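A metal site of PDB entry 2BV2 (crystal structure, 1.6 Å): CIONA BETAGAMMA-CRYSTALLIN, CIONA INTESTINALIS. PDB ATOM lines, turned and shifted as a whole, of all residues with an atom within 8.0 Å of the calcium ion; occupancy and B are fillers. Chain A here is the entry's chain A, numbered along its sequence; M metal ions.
The backbone NH of Asp 48 is in hydrogen-bond range of the backbone carbonyl oxygen of Pro 55. N of Ser 78 is in hydrogen-bond range of O of Phe 47 (2.8 Å). The side-chain amide oxygen (OD1) of Asn 31 sits close to the side-chain hydroxyl (OG) of Ser 78 (2.7 Å). OD2 of Asp 32 lies within hydrogen-bond range of ND2 of Asn 31. The backbone NH (N) of Asp 32 sits at hydrogen-bond distance from the backbone carbonyl oxygen (O) of Leu 77 (3.1 Å). The backbone carbonyl oxygen (O) of Ser 78 is in hydrogen-bond range of the backbone NH (N) of Leu 25 (2.8 Å).
OG of Ser 78 is bound to the calcium ion. The calcium ion is bound by O of Asp 48 (2.3 Å). O of Glu 76 binds the calcium ion, at 2.4 Å. OD1 of Asp 32 binds the calcium ion (2.5 Å). The calcium ion is bound by OE1 of Glu 76. The calcium ion has five donor atoms within binding distance.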
ATOM      1  N   LEU A  25     -20.390  14.407 -13.991  1.00  0.00           N
ATOM      2  CA  LEU A  25     -21.662  15.068 -14.327  1.00  0.00           C
ATOM      3  C   LEU A  25     -22.797  14.121 -14.681  1.00  0.00           C
ATOM      4  O   LEU A  25     -23.936  14.544 -14.668  1.00  0.00           O
ATOM      5  CB  LEU A  25     -21.487  16.117 -15.421  1.00  0.00           C
ATOM      6  CG  LEU A  25     -20.810  17.423 -14.989  1.00  0.00           C
ATOM      7  CD1 LEU A  25     -20.553  18.238 -16.194  1.00  0.00           C
ATOM      8  CD2 LEU A  25     -21.644  18.246 -13.994  1.00  0.00           C
ATOM      9  N   ASN A  26     -22.485  12.871 -15.007  1.00  0.00           N
ATOM     10  CA  ASN A  26     -23.522  11.841 -15.237  1.00  0.00           C
ATOM     11  C   ASN A  26     -24.482  11.661 -14.070  1.00  0.00           C
ATOM     12  O   ASN A  26     -25.648  11.296 -14.265  1.00  0.00           O
ATOM     13  CB  ASN A  26     -22.916  10.492 -15.544  1.00  0.00           C
ATOM     14  CG  ASN A  26     -22.358  10.384 -16.941  1.00  0.00           C
ATOM     15  OD1 ASN A  26     -23.091  10.463 -17.938  1.00  0.00           O
ATOM     16  ND2 ASN A  26     -21.056  10.151 -17.039  1.00  0.00           N
ATOM     17  N   PHE A  30     -25.840  15.389 -16.857  1.00  0.00           N
ATOM     18  CA  PHE A  30     -25.259  16.559 -17.509  1.00  0.00           C
ATOM     19  C   PHE A  30     -23.880  16.288 -18.128  1.00  0.00           C
ATOM     20  O   PHE A  30     -23.114  17.211 -18.407  1.00  0.00           O
ATOM     21  CB  PHE A  30     -25.220  17.742 -16.544  1.00  0.00           C
ATOM     22  CG  PHE A  30     -26.229  18.801 -16.852  1.00  0.00           C
ATOM     23  CD1 PHE A  30     -27.561  18.608 -16.540  1.00  0.00           C
ATOM     24  CD2 PHE A  30     -25.841  20.003 -17.449  1.00  0.00           C
ATOM     25  CE1 PHE A  30     -28.495  19.578 -16.850  1.00  0.00           C
ATOM     26  CE2 PHE A  30     -26.778  20.959 -17.763  1.00  0.00           C
ATOM     27  CZ  PHE A  30     -28.097  20.748 -17.451  1.00  0.00           C
ATOM     28  N   ASN A  31     -23.569  15.026 -18.330  1.00  0.00           N
ATOM     29  CA  ASN A  31     -22.340  14.664 -19.001  1.00  0.00           C
ATOM     30  C   ASN A  31     -22.457  14.885 -20.489  1.00  0.00           C
ATOM     31  O   ASN A  31     -23.408  14.437 -21.127  1.00  0.00           O
ATOM     32  CB  ASN A  31     -21.966  13.206 -18.741  1.00  0.00           C
ATOM     33  CG  ASN A  31     -20.538  12.903 -19.142  1.00  0.00           C
ATOM     34  OD1 ASN A  31     -19.607  13.520 -18.631  1.00  0.00           O
ATOM     35  ND2 ASN A  31     -20.363  11.965 -20.073  1.00  0.00           N
ATOM     36  N   ASP A  32     -21.468  15.576 -21.048  1.00  0.00           N
ATOM     37  CA  ASP A  32     -21.323  15.778 -22.485  1.00  0.00           C
ATOM     38  C   ASP A  32     -22.528  16.429 -23.156  1.00  0.00           C
ATOM     39  O   ASP A  32     -22.892  16.074 -24.280  1.00  0.00           O
ATOM     40  CB  ASP A  32     -20.933  14.486 -23.188  1.00  0.00           C
ATOM     41  CG  ASP A  32     -19.555  13.997 -22.788  1.00  0.00           C
ATOM     42  OD1 ASP A  32     -18.819  14.742 -22.128  1.00  0.00           O
ATOM     43  OD2 ASP A  32     -19.198  12.857 -23.148  1.00  0.00           O
ATOM     44  N   ILE A  33     -23.145  17.384 -22.458  1.00  0.00           N
ATOM     45  CA  ILE A  33     -24.187  18.198 -23.071  1.00  0.00           C
ATOM     46  C   ILE A  33     -24.033  19.694 -22.910  1.00  0.00           C
ATOM     47  O   ILE A  33     -24.789  20.421 -23.530  1.00  0.00           O
ATOM     48  CB  ILE A  33     -25.609  17.847 -22.543  1.00  0.00           C
ATOM     49  CG1 ILE A  33     -25.765  18.181 -21.065  1.00  0.00           C
ATOM     50  CG2 ILE A  33     -25.924  16.383 -22.800  1.00  0.00           C
ATOM     51  CD1 ILE A  33     -27.204  18.053 -20.603  1.00  0.00           C
ATOM     52  N   PHE A  47     -13.816  20.552 -16.627  1.00  0.00           N
ATOM     53  CA  PHE A  47     -12.958  19.552 -17.235  1.00  0.00           C
ATOM     54  C   PHE A  47     -13.730  18.702 -18.231  1.00  0.00           C
ATOM     55  O   PHE A  47     -14.871  18.353 -17.986  1.00  0.00           O
ATOM     56  CB  PHE A  47     -12.437  18.615 -16.150  1.00  0.00           C
ATOM     57  CG  PHE A  47     -11.642  19.289 -15.077  1.00  0.00           C
ATOM     58  CD1 PHE A  47     -10.256  19.272 -15.121  1.00  0.00           C
ATOM     59  CD2 PHE A  47     -12.260  19.859 -13.973  1.00  0.00           C
ATOM     60  CE1 PHE A  47      -9.516  19.875 -14.119  1.00  0.00           C
ATOM     61  CE2 PHE A  47     -11.533  20.457 -12.973  1.00  0.00           C
ATOM     62  CZ  PHE A  47     -10.164  20.460 -13.041  1.00  0.00           C
ATOM     63  N   ASP A  48     -13.066  18.324 -19.323  1.00  0.00           N
ATOM     64  CA  ASP A  48     -13.658  17.436 -20.323  1.00  0.00           C
ATOM     65  C   ASP A  48     -13.634  15.927 -19.996  1.00  0.00           C
ATOM     66  O   ASP A  48     -14.339  15.164 -20.666  1.00  0.00           O
ATOM     67  CB  ASP A  48     -13.027  17.663 -21.694  1.00  0.00           C
ATOM     68  CG  ASP A  48     -13.411  19.003 -22.287  1.00  0.00           C
ATOM     69  OD1 ASP A  48     -14.302  19.680 -21.735  1.00  0.00           O
ATOM     70  OD2 ASP A  48     -12.815  19.391 -23.319  1.00  0.00           O
ATOM     71  N   ASP A  49     -12.851  15.499 -19.005  1.00  0.00           N
ATOM     72  CA  ASP A  49     -12.956  14.143 -18.481  1.00  0.00           C
ATOM     73  C   ASP A  49     -13.578  14.175 -17.095  1.00  0.00           C
ATOM     74  O   ASP A  49     -13.646  15.231 -16.448  1.00  0.00           O
ATOM     75  CB  ASP A  49     -11.597  13.419 -18.400  1.00  0.00           C
ATOM     76  CG  ASP A  49     -10.986  13.116 -19.769  1.00  0.00           C
ATOM     77  OD1 ASP A  49     -11.664  13.324 -20.817  1.00  0.00           O
ATOM     78  OD2 ASP A  49      -9.800  12.657 -19.766  1.00  0.00           O
ATOM     79  N   GLU A  50     -14.039  13.006 -16.662  1.00  0.00           N
ATOM     80  CA  GLU A  50     -14.536  12.834 -15.301  1.00  0.00           C
ATOM     81  C   GLU A  50     -13.338  12.895 -14.335  1.00  0.00           C
ATOM     82  O   GLU A  50     -12.185  12.744 -14.743  1.00  0.00           O
ATOM     83  CB  GLU A  50     -15.257  11.498 -15.147  1.00  0.00           C
ATOM     84  CG  GLU A  50     -16.470  11.335 -16.052  1.00  0.00           C
ATOM     85  CD  GLU A  50     -17.143   9.985 -15.881  1.00  0.00           C
ATOM     86  OE1 GLU A  50     -17.913   9.560 -16.789  1.00  0.00           O
ATOM     87  OE2 GLU A  50     -16.890   9.337 -14.854  1.00  0.00           O
ATOM     88  N   SER A  53     -10.148  15.893 -14.551  1.00  0.00           N
ATOM     89  CA  SER A  53      -9.035  15.487 -15.383  1.00  0.00           C
ATOM     90  C   SER A  53      -9.431  15.703 -16.821  1.00  0.00           C
ATOM     91  O   SER A  53     -10.574  16.067 -17.073  1.00  0.00           O
ATOM     92  CB  SER A  53      -8.692  14.023 -15.115  1.00  0.00           C
ATOM     93  OG  SER A  53      -9.681  13.150 -15.625  1.00  0.00           O
ATOM     94  N   PRO A  55      -8.787  17.863 -20.559  1.00  0.00           N
ATOM     95  CA  PRO A  55      -8.731  19.289 -20.842  1.00  0.00           C
ATOM     96  C   PRO A  55      -9.485  20.112 -19.781  1.00  0.00           C
ATOM     97  O   PRO A  55     -10.617  19.784 -19.449  1.00  0.00           O
ATOM     98  CB  PRO A  55      -9.417  19.387 -22.202  1.00  0.00           C
ATOM     99  CG  PRO A  55      -9.070  18.109 -22.860  1.00  0.00           C
ATOM    100  CD  PRO A  55      -9.065  17.066 -21.766  1.00  0.00           C
ATOM    101  N   ASP A  74     -17.843  21.879 -27.543  1.00  0.00           N
ATOM    102  CA  ASP A  74     -19.259  21.700 -27.249  1.00  0.00           C
ATOM    103  C   ASP A  74     -19.503  20.288 -26.777  1.00  0.00           C
ATOM    104  O   ASP A  74     -18.879  19.369 -27.279  1.00  0.00           O
ATOM    105  CB  ASP A  74     -20.105  21.969 -28.494  1.00  0.00           C
ATOM    106  CG  ASP A  74     -21.577  22.012 -28.177  1.00  0.00           C
ATOM    107  OD1 ASP A  74     -21.932  22.683 -27.213  1.00  0.00           O
ATOM    108  OD2 ASP A  74     -22.366  21.336 -28.877  1.00  0.00           O
ATOM    109  N   ASP A  75     -20.409  20.134 -25.799  1.00  0.00           N
ATOM    110  CA  ASP A  75     -20.891  18.808 -25.427  1.00  0.00           C
ATOM    111  C   ASP A  75     -19.746  17.896 -24.958  1.00  0.00           C
ATOM    112  O   ASP A  75     -19.673  16.727 -25.368  1.00  0.00           O
ATOM    113  CB  ASP A  75     -21.660  18.144 -26.586  1.00  0.00           C
ATOM    114  CG  ASP A  75     -23.119  18.543 -26.642  1.00  0.00           C
ATOM    115  OD1 ASP A  75     -23.485  19.554 -26.015  1.00  0.00           O
ATOM    116  OD2 ASP A  75     -23.918  17.811 -27.307  1.00  0.00           O
ATOM    117  N   GLU A  76     -18.886  18.437 -24.104  1.00  0.00           N
ATOM    118  CA  GLU A  76     -17.716  17.730 -23.600  1.00  0.00           C
ATOM    119  C   GLU A  76     -17.421  17.854 -22.107  1.00  0.00           C
ATOM    120  O   GLU A  76     -16.612  17.102 -21.572  1.00  0.00           O
ATOM    121  CB  GLU A  76     -16.460  18.136 -24.375  1.00  0.00           C
ATOM    122  CG  GLU A  76     -15.339  17.110 -24.349  1.00  0.00           C
ATOM    123  CD  GLU A  76     -15.803  15.740 -24.753  1.00  0.00           C
ATOM    124  OE1 GLU A  76     -15.630  14.770 -23.961  1.00  0.00           O
ATOM    125  OE2 GLU A  76     -16.380  15.657 -25.870  1.00  0.00           O
ATOM    126  N   LEU A  77     -18.067  18.759 -21.403  1.00  0.00           N
ATOM    127  CA  LEU A  77     -17.765  18.874 -19.974  1.00  0.00           C
ATOM    128  C   LEU A  77     -18.226  17.606 -19.257  1.00  0.00           C
ATOM    129  O   LEU A  77     -19.317  17.111 -19.510  1.00  0.00           O
ATOM    130  CB  LEU A  77     -18.410  20.112 -19.352  1.00  0.00           C
ATOM    131  CG  LEU A  77     -17.763  21.417 -19.857  1.00  0.00           C
ATOM    132  CD1 LEU A  77     -18.376  22.597 -19.174  1.00  0.00           C
ATOM    133  CD2 LEU A  77     -16.249  21.412 -19.652  1.00  0.00           C
ATOM    134  N   SER A  78     -17.381  17.092 -18.377  1.00  0.00           N
ATOM    135  CA  SER A  78     -17.720  15.902 -17.597  1.00  0.00           C
ATOM    136  C   SER A  78     -17.562  16.047 -16.092  1.00  0.00           C
ATOM    137  O   SER A  78     -18.128  15.233 -15.337  1.00  0.00           O
ATOM    138  CB  SER A  78     -16.916  14.715 -18.100  1.00  0.00           C
ATOM    139  OG  SER A  78     -17.220  14.451 -19.451  1.00  0.00           O
ATOM    140  N   SER A  79     -16.797  17.035 -15.641  1.00  0.00           N
ATOM    141  CA  SER A  79     -16.651  17.296 -14.201  1.00  0.00           C
ATOM    142  C   SER A  79     -16.316  18.779 -13.967  1.00  0.00           C
ATOM    143  O   SER A  79     -15.862  19.442 -14.883  1.00  0.00           O
ATOM    144  CB  SER A  79     -15.580  16.387 -13.570  1.00  0.00           C
ATOM    145  OG  SER A  79     -14.281  16.635 -14.110  1.00  0.00           O
HETATM  146 CA    CA M   1     -16.427  14.717 -21.539  1.00  0.00          CA
